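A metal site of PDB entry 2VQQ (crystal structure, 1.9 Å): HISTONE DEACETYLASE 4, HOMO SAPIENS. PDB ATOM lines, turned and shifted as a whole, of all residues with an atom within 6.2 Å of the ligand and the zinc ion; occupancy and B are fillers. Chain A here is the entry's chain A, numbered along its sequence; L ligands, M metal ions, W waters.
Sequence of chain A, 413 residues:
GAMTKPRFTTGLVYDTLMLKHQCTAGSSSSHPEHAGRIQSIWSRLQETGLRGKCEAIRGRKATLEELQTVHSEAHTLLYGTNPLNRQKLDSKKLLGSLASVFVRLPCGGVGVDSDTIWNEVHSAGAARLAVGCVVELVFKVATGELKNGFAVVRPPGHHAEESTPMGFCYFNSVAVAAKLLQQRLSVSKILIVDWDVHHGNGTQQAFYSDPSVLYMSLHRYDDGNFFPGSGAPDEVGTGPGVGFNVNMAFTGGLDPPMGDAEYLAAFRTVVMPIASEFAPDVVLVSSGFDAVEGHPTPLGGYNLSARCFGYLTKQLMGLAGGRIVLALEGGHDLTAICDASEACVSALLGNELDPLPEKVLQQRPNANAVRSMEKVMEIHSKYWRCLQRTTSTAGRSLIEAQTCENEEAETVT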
ATOM      1  N   ARG A  37      -7.761  27.416  17.480  1.00  0.00           N
ATOM      2  CA  ARG A  37      -6.963  27.056  18.673  1.00  0.00           C
ATOM      3  C   ARG A  37      -5.461  26.978  18.394  1.00  0.00           C
ATOM      4  O   ARG A  37      -4.692  27.704  19.020  1.00  0.00           O
ATOM      5  CB  ARG A  37      -7.450  25.716  19.244  1.00  0.00           C
ATOM      6  CG  ARG A  37      -8.862  25.765  19.838  1.00  0.00           C
ATOM      7  CD  ARG A  37      -9.218  24.454  20.553  1.00  0.00           C
ATOM      8  NE  ARG A  37      -8.815  23.294  19.763  1.00  0.00           N
ATOM      9  CZ  ARG A  37      -8.080  22.269  20.192  1.00  0.00           C
ATOM     10  NH1 ARG A  37      -7.682  22.149  21.459  1.00  0.00           N
ATOM     11  NH2 ARG A  37      -7.776  21.312  19.340  1.00  0.00           N
ATOM     12  N   PRO A 156      -7.393  16.557  18.423  1.00  0.00           N
ATOM     13  CA  PRO A 156      -6.875  15.721  19.512  1.00  0.00           C
ATOM     14  C   PRO A 156      -6.943  14.233  19.150  1.00  0.00           C
ATOM     15  O   PRO A 156      -7.601  13.858  18.174  1.00  0.00           O
ATOM     16  CB  PRO A 156      -7.799  16.053  20.695  1.00  0.00           C
ATOM     17  CG  PRO A 156      -9.057  16.529  20.066  1.00  0.00           C
ATOM     18  CD  PRO A 156      -8.648  17.238  18.817  1.00  0.00           C
ATOM     19  N   GLY A 157      -6.246  13.400  19.919  1.00  0.00           N
ATOM     20  CA  GLY A 157      -6.135  11.975  19.645  1.00  0.00           C
ATOM     21  C   GLY A 157      -6.588  11.001  20.716  1.00  0.00           C
ATOM     22  O   GLY A 157      -6.874   9.843  20.420  1.00  0.00           O
ATOM     23  N   HIS A 158      -6.644  11.455  21.970  1.00  0.00           N
ATOM     24  CA  HIS A 158      -6.694  10.527  23.102  1.00  0.00           C
ATOM     25  C   HIS A 158      -7.995   9.723  23.262  1.00  0.00           C
ATOM     26  O   HIS A 158      -8.002   8.719  23.986  1.00  0.00           O
ATOM     27  CB  HIS A 158      -6.248  11.208  24.408  1.00  0.00           C
ATOM     28  CG  HIS A 158      -7.263  12.144  25.025  1.00  0.00           C
ATOM     29  ND1 HIS A 158      -7.341  12.343  26.379  1.00  0.00           N
ATOM     30  CD2 HIS A 158      -8.216  12.932  24.471  1.00  0.00           C
ATOM     31  CE1 HIS A 158      -8.303  13.213  26.644  1.00  0.00           C
ATOM     32  NE2 HIS A 158      -8.850  13.587  25.502  1.00  0.00           N
ATOM     33  N   HIS A 159      -9.077  10.107  22.570  1.00  0.00           N
ATOM     34  CA  HIS A 159     -10.318   9.304  22.600  1.00  0.00           C
ATOM     35  C   HIS A 159     -10.401   8.230  21.509  1.00  0.00           C
ATOM     36  O   HIS A 159     -11.209   7.309  21.626  1.00  0.00           O
ATOM     37  CB  HIS A 159     -11.574  10.191  22.522  1.00  0.00           C
ATOM     38  CG  HIS A 159     -11.731  11.133  23.680  1.00  0.00           C
ATOM     39  ND1 HIS A 159     -11.771  10.706  24.990  1.00  0.00           N
ATOM     40  CD2 HIS A 159     -11.898  12.477  23.714  1.00  0.00           C
ATOM     41  CE1 HIS A 159     -11.933  11.753  25.783  1.00  0.00           C
ATOM     42  NE2 HIS A 159     -12.006  12.840  25.042  1.00  0.00           N
ATOM     43  N   MET A 166     -13.940   8.966  17.833  1.00  0.00           N
ATOM     44  CA  MET A 166     -14.911   9.536  18.771  1.00  0.00           C
ATOM     45  C   MET A 166     -14.320  10.738  19.469  1.00  0.00           C
ATOM     46  O   MET A 166     -13.101  10.908  19.499  1.00  0.00           O
ATOM     47  CB  MET A 166     -15.358   8.511  19.812  1.00  0.00           C
ATOM     48  CG  MET A 166     -14.228   7.804  20.551  1.00  0.00           C
ATOM     49  SD  MET A 166     -14.836   6.628  21.799  1.00  0.00           S
ATOM     50  CE  MET A 166     -15.161   7.737  23.131  1.00  0.00           C
ATOM     51  N   GLY A 167     -15.191  11.570  20.034  1.00  0.00           N
ATOM     52  CA  GLY A 167     -14.764  12.757  20.778  1.00  0.00           C
ATOM     53  C   GLY A 167     -13.802  13.629  19.993  1.00  0.00           C
ATOM     54  O   GLY A 167     -12.783  14.061  20.528  1.00  0.00           O
ATOM     55  N   PHE A 168     -14.125  13.873  18.721  1.00  0.00           N
ATOM     56  CA  PHE A 168     -13.293  14.701  17.820  1.00  0.00           C
ATOM     57  C   PHE A 168     -11.943  14.065  17.410  1.00  0.00           C
ATOM     58  O   PHE A 168     -11.154  14.723  16.727  1.00  0.00           O
ATOM     59  CB  PHE A 168     -13.023  16.105  18.407  1.00  0.00           C
ATOM     60  CG  PHE A 168     -14.242  16.803  18.949  1.00  0.00           C
ATOM     61  CD1 PHE A 168     -14.316  17.153  20.282  1.00  0.00           C
ATOM     62  CD2 PHE A 168     -15.289  17.144  18.125  1.00  0.00           C
ATOM     63  CE1 PHE A 168     -15.428  17.819  20.800  1.00  0.00           C
ATOM     64  CE2 PHE A 168     -16.412  17.805  18.624  1.00  0.00           C
ATOM     65  CZ  PHE A 168     -16.473  18.139  19.968  1.00  0.00           C
ATOM     66  N   CYS A 169     -11.703  12.820  17.797  1.00  0.00           N
ATOM     67  CA  CYS A 169     -10.430  12.126  17.574  1.00  0.00           C
ATOM     68  C   CYS A 169     -10.558  11.029  16.519  1.00  0.00           C
ATOM     69  O   CYS A 169     -11.453  10.188  16.586  1.00  0.00           O
ATOM     70  CB  CYS A 169      -9.894  11.516  18.875  1.00  0.00           C
ATOM     71  SG  CYS A 169      -9.763  12.673  20.279  1.00  0.00           S
ATOM     72  N   ASP A 196      -5.698  16.304  30.288  1.00  0.00           N
ATOM     73  CA  ASP A 196      -6.984  16.734  29.736  1.00  0.00           C
ATOM     74  C   ASP A 196      -8.053  16.388  30.793  1.00  0.00           C
ATOM     75  O   ASP A 196      -7.932  15.375  31.501  1.00  0.00           O
ATOM     76  CB  ASP A 196      -7.233  16.023  28.401  1.00  0.00           C
ATOM     77  CG  ASP A 196      -8.430  16.577  27.631  1.00  0.00           C
ATOM     78  OD1 ASP A 196      -8.241  17.346  26.660  1.00  0.00           O
ATOM     79  OD2 ASP A 196      -9.569  16.269  28.013  1.00  0.00           O
ATOM     80  N   VAL A 197      -9.086  17.211  30.903  1.00  0.00           N
ATOM     81  CA  VAL A 197     -10.119  16.987  31.925  1.00  0.00           C
ATOM     82  C   VAL A 197     -10.966  15.716  31.652  1.00  0.00           C
ATOM     83  O   VAL A 197     -11.645  15.220  32.554  1.00  0.00           O
ATOM     84  CB  VAL A 197     -11.003  18.234  32.137  1.00  0.00           C
ATOM     85  CG1 VAL A 197     -12.124  18.326  31.096  1.00  0.00           C
ATOM     86  CG2 VAL A 197     -11.587  18.258  33.584  1.00  0.00           C
ATOM     87  N   HIS A 198     -10.925  15.188  30.427  1.00  0.00           N
ATOM     88  CA  HIS A 198     -11.659  13.965  30.084  1.00  0.00           C
ATOM     89  C   HIS A 198     -10.723  12.750  30.019  1.00  0.00           C
ATOM     90  O   HIS A 198      -9.562  12.872  29.615  1.00  0.00           O
ATOM     91  CB  HIS A 198     -12.395  14.135  28.746  1.00  0.00           C
ATOM     92  CG  HIS A 198     -13.310  15.317  28.711  1.00  0.00           C
ATOM     93  ND1 HIS A 198     -12.898  16.569  28.306  1.00  0.00           N
ATOM     94  CD2 HIS A 198     -14.607  15.440  29.072  1.00  0.00           C
ATOM     95  CE1 HIS A 198     -13.911  17.409  28.401  1.00  0.00           C
ATOM     96  NE2 HIS A 198     -14.948  16.753  28.877  1.00  0.00           N
ATOM     97  N   HIS A 199     -11.217  11.578  30.429  1.00  0.00           N
ATOM     98  CA  HIS A 199     -10.431  10.352  30.417  1.00  0.00           C
ATOM     99  C   HIS A 199      -9.952   9.985  29.000  1.00  0.00           C
ATOM    100  O   HIS A 199     -10.732   9.977  28.058  1.00  0.00           O
ATOM    101  CB  HIS A 199     -11.262   9.196  30.972  1.00  0.00           C
ATOM    102  CG  HIS A 199     -10.537   7.897  31.009  1.00  0.00           C
ATOM    103  ND1 HIS A 199     -10.947   6.784  30.304  1.00  0.00           N
ATOM    104  CD2 HIS A 199      -9.404   7.524  31.660  1.00  0.00           C
ATOM    105  CE1 HIS A 199     -10.110   5.793  30.515  1.00  0.00           C
ATOM    106  NE2 HIS A 199      -9.162   6.212  31.339  1.00  0.00           N
ATOM    107  N   PHE A 226     -19.553  11.433  33.408  1.00  0.00           N
ATOM    108  CA  PHE A 226     -18.907  12.511  32.672  1.00  0.00           C
ATOM    109  C   PHE A 226     -18.204  11.920  31.436  1.00  0.00           C
ATOM    110  O   PHE A 226     -17.648  10.832  31.514  1.00  0.00           O
ATOM    111  CB  PHE A 226     -17.913  13.229  33.594  1.00  0.00           C
ATOM    112  CG  PHE A 226     -17.434  14.544  33.064  1.00  0.00           C
ATOM    113  CD1 PHE A 226     -18.284  15.640  33.019  1.00  0.00           C
ATOM    114  CD2 PHE A 226     -16.126  14.698  32.615  1.00  0.00           C
ATOM    115  CE1 PHE A 226     -17.848  16.869  32.516  1.00  0.00           C
ATOM    116  CE2 PHE A 226     -15.677  15.909  32.123  1.00  0.00           C
ATOM    117  CZ  PHE A 226     -16.555  17.006  32.068  1.00  0.00           C
ATOM    118  N   PHE A 227     -18.272  12.622  30.297  1.00  0.00           N
ATOM    119  CA  PHE A 227     -17.721  12.100  29.026  1.00  0.00           C
ATOM    120  C   PHE A 227     -16.236  11.721  29.185  1.00  0.00           C
ATOM    121  O   PHE A 227     -15.472  12.489  29.758  1.00  0.00           O
ATOM    122  CB  PHE A 227     -17.891  13.144  27.904  1.00  0.00           C
ATOM    123  CG  PHE A 227     -17.409  12.659  26.551  1.00  0.00           C
ATOM    124  CD1 PHE A 227     -18.272  12.006  25.671  1.00  0.00           C
ATOM    125  CD2 PHE A 227     -16.086  12.853  26.154  1.00  0.00           C
ATOM    126  CE1 PHE A 227     -17.835  11.548  24.438  1.00  0.00           C
ATOM    127  CE2 PHE A 227     -15.638  12.402  24.918  1.00  0.00           C
ATOM    128  CZ  PHE A 227     -16.505  11.749  24.051  1.00  0.00           C
ATOM    129  N   GLY A 288      -4.185  18.358  27.357  1.00  0.00           N
ATOM    130  CA  GLY A 288      -5.410  19.104  27.164  1.00  0.00           C
ATOM    131  C   GLY A 288      -5.464  20.162  28.244  1.00  0.00           C
ATOM    132  O   GLY A 288      -4.952  19.956  29.352  1.00  0.00           O
ATOM    133  N   ASP A 290      -8.575  21.860  29.008  1.00  0.00           N
ATOM    134  CA  ASP A 290      -9.995  22.093  29.345  1.00  0.00           C
ATOM    135  C   ASP A 290     -10.304  22.086  30.864  1.00  0.00           C
ATOM    136  O   ASP A 290     -11.425  22.380  31.257  1.00  0.00           O
ATOM    137  CB  ASP A 290     -10.962  21.139  28.565  1.00  0.00           C
ATOM    138  CG  ASP A 290     -10.484  19.688  28.471  1.00  0.00           C
ATOM    139  OD1 ASP A 290      -9.492  19.275  29.138  1.00  0.00           O
ATOM    140  OD2 ASP A 290     -11.137  18.939  27.683  1.00  0.00           O
ATOM    141  N   PRO A 298     -20.216  21.262  31.346  1.00  0.00           N
ATOM    142  CA  PRO A 298     -19.995  19.977  30.645  1.00  0.00           C
ATOM    143  C   PRO A 298     -18.678  19.856  29.841  1.00  0.00           C
ATOM    144  O   PRO A 298     -18.043  18.794  29.858  1.00  0.00           O
ATOM    145  CB  PRO A 298     -21.213  19.859  29.717  1.00  0.00           C
ATOM    146  CG  PRO A 298     -21.766  21.254  29.587  1.00  0.00           C
ATOM    147  CD  PRO A 298     -21.010  22.190  30.525  1.00  0.00           C
ATOM    148  N   LEU A 299     -18.269  20.929  29.164  1.00  0.00           N
ATOM    149  CA  LEU A 299     -17.027  20.946  28.393  1.00  0.00           C
ATOM    150  C   LEU A 299     -15.889  21.521  29.239  1.00  0.00           C
ATOM    151  O   LEU A 299     -15.116  22.371  28.784  1.00  0.00           O
ATOM    152  CB  LEU A 299     -17.202  21.800  27.133  1.00  0.00           C
ATOM    153  CG  LEU A 299     -18.352  21.449  26.181  1.00  0.00           C
ATOM    154  CD1 LEU A 299     -18.519  22.526  25.114  1.00  0.00           C
ATOM    155  CD2 LEU A 299     -18.110  20.081  25.558  1.00  0.00           C
ATOM    156  N   GLU A 329      -4.161  18.353  23.383  1.00  0.00           N
ATOM    157  CA  GLU A 329      -5.369  17.558  23.230  1.00  0.00           C
ATOM    158  C   GLU A 329      -6.562  18.532  23.209  1.00  0.00           C
ATOM    159  O   GLU A 329      -6.664  19.320  22.271  1.00  0.00           O
ATOM    160  CB  GLU A 329      -5.468  16.502  24.332  1.00  0.00           C
ATOM    161  CG  GLU A 329      -4.300  15.468  24.312  1.00  0.00           C
ATOM    162  CD  GLU A 329      -4.477  14.339  23.290  1.00  0.00           C
ATOM    163  OE1 GLU A 329      -5.457  14.328  22.518  1.00  0.00           O
ATOM    164  OE2 GLU A 329      -3.597  13.446  23.273  1.00  0.00           O
ATOM    165  N   GLY A 330      -7.423  18.496  24.225  1.00  0.00           N
ATOM    166  CA  GLY A 330      -8.589  19.389  24.314  1.00  0.00           C
ATOM    167  C   GLY A 330      -8.313  20.723  24.990  1.00  0.00           C
ATOM    168  O   GLY A 330      -7.163  21.084  25.237  1.00  0.00           O
ATOM    169  N   GLY A 331      -9.390  21.431  25.312  1.00  0.00           N
ATOM    170  CA  GLY A 331      -9.366  22.849  25.671  1.00  0.00           C
ATOM    171  C   GLY A 331      -9.877  23.665  24.493  1.00  0.00           C
ATOM    172  O   GLY A 331      -9.628  23.319  23.357  1.00  0.00           O
ATOM    173  N   HIS A 332     -10.624  24.731  24.745  1.00  0.00           N
ATOM    174  CA  HIS A 332     -11.196  25.531  23.659  1.00  0.00           C
ATOM    175  C   HIS A 332     -11.285  27.037  23.914  1.00  0.00           C
ATOM    176  O   HIS A 332     -11.291  27.815  22.965  1.00  0.00           O
ATOM    177  CB  HIS A 332     -12.569  24.965  23.241  1.00  0.00           C
ATOM    178  CG  HIS A 332     -13.489  24.704  24.384  1.00  0.00           C
ATOM    179  ND1 HIS A 332     -14.341  25.665  24.901  1.00  0.00           N
ATOM    180  CD2 HIS A 332     -13.708  23.577  25.118  1.00  0.00           C
ATOM    181  CE1 HIS A 332     -15.034  25.149  25.895  1.00  0.00           C
ATOM    182  NE2 HIS A 332     -14.667  23.888  26.048  1.00  0.00           N
HETATM  183  C1  LIG L   1     -23.734  18.912  23.073  1.00  0.00           C
HETATM  184  C2  LIG L   1     -24.814  19.524  23.720  1.00  0.00           C
HETATM  185  C3  LIG L   1     -24.631  20.053  24.993  1.00  0.00           C
HETATM  186  C4  LIG L   1     -23.387  19.945  25.620  1.00  0.00           C
HETATM  187  C5  LIG L   1     -22.315  19.339  24.956  1.00  0.00           C
HETATM  188  C6  LIG L   1     -22.478  18.826  23.668  1.00  0.00           C
HETATM  189  C7  LIG L   1     -21.429  18.179  22.978  1.00  0.00           C
HETATM  190  C8  LIG L   1     -21.102  18.184  21.691  1.00  0.00           C
HETATM  191  N1  LIG L   1     -20.046  17.391  21.477  1.00  0.00           N
HETATM  192  C9  LIG L   1     -19.664  16.836  22.636  1.00  0.00           C
HETATM  193  C10 LIG L   1     -18.508  15.836  22.951  1.00  0.00           C
HETATM  194  N2  LIG L   1     -20.549  17.337  23.616  1.00  0.00           N
HETATM  195  C11 LIG L   1     -20.473  16.992  25.037  1.00  0.00           C
HETATM  196  C12 LIG L   1     -19.550  15.851  25.264  1.00  0.00           C
HETATM  197  N3  LIG L   1     -18.342  15.914  24.408  1.00  0.00           N
HETATM  198  C13 LIG L   1     -17.201  16.156  25.067  1.00  0.00           C
HETATM  199  O1  LIG L   1     -17.285  16.217  26.300  1.00  0.00           O
HETATM  200  C14 LIG L   1     -15.791  16.139  24.541  1.00  0.00           C
HETATM  201  S1  LIG L   1     -14.547  16.876  25.356  1.00  0.00           S
HETATM  202  C15 LIG L   1     -15.301  15.377  23.553  1.00  0.00           C
HETATM  203  C16 LIG L   1     -13.955  15.458  23.406  1.00  0.00           C
HETATM  204  C17 LIG L   1     -13.353  16.243  24.343  1.00  0.00           C
HETATM  205  C18 LIG L   1     -11.870  16.533  24.532  1.00  0.00           C
HETATM  206  C19 LIG L   1     -10.982  16.535  23.276  1.00  0.00           C
HETATM  207  F1  LIG L   1      -9.752  16.618  23.742  1.00  0.00           F
HETATM  208  F2  LIG L   1     -11.112  15.415  22.557  1.00  0.00           F
HETATM  209  F3  LIG L   1     -11.224  17.598  22.512  1.00  0.00           F
HETATM  210  O2  LIG L   1     -11.296  15.496  25.428  1.00  0.00           O
HETATM  211  O3  LIG L   1     -11.721  17.751  25.263  1.00  0.00           O
HETATM  212 ZN    ZN M   1     -11.123  17.143  27.072  1.00  0.00          ZN
HETATM  213  O   HOH W   1     -11.880  20.133  24.491  1.00  0.00           O
HETATM  214  O   HOH W   2     -18.283  16.424  28.780  1.00  0.00           O
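NE2 of His 159 lies close to O2 of the ligand (2.8 Å).
A ring nitrogen (NE2) of His 158 lies close to an oxygen (O2) of the ligand (3.1 Å).
The backbone NH (N) of Val 197 sits at hydrogen-bond distance from the side-chain carboxylate (OD1) of Asp 290 (2.7 Å).
The backbone NH (N) of Gly 330 is in hydrogen-bond range of the side-chain carboxylate (OD1) of Asp 196, at 2.8 Å.
A ring nitrogen (NE2) of His 158 is in hydrogen-bond range of a ring nitrogen (NE2) of His 159 (3.3 Å).
The backbone carbonyl oxygen of Gly 167 lies within hydrogen-bond range of the side-chain sulfur of Cys 169 (3.3 Å).
The backbone NH (N) of His 158 is in hydrogen-bond range of the side-chain carboxylate (OE1) of Glu 329, at 3.2 Å.
O of Pro 156 sits at hydrogen-bond distance from SG of Cys 169.
The backbone NH (N) of Gly 157 sits at hydrogen-bond distance from the side-chain carboxylate (OE1) of Glu 329, at 2.9 Å.
O of Leu 299 lies within hydrogen-bond range of NE2 of His 332 (3.2 Å).
The backbone carbonyl oxygen of Gly 167 lies close to a fluorine (F2) of the ligand (3.0 Å).
A fluorine (F1) of the ligand lies close to the backbone NH (N) of Gly 330 (3.0 Å).
Pro 156 touches the ligand.
Phe 168 touches the ligand (CD1 to C16, 3.6 Å).
SG of Cys 169 touches F2 of the ligand, 3.8 Å away.
CE2 of Phe 227 touches C15 of the ligand (3.3 Å).
Leu 299 touches the ligand (CD2 to C11, 3.9 Å).
Glu 329 touches the ligand (C to F1, 3.8 Å).
Hydrophobic or aromatic side chains that line the ligand: Pro 156, His 158, His 159, Phe 168, His 198, Phe 227 and Leu 299.
Of the 23 residues printed, 13 come within 4 Å of the ligand.
The nearest printed residue that does not touch the ligand is Gly 331 (4.4 Å).
Of the 23 residues printed, 3 come within 4 Å of the zinc ion.
The nearest printed residue that does not touch the zinc ion is Val 197 (4.3 Å).
The zinc ion is bound by the side-chain carboxylate of Asp 290, an oxygen (O3) of the ligand, the side-chain carboxylate of Asp 196, a ring nitrogen (ND1) of His 198 and an oxygen (O2) of the ligand.
Water W2 lies within hydrogen-bond range of O of Pro 298 (2.6 Å), O1 of the ligand (2.7 Å) and NE2 of His 198 (3.4 Å).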
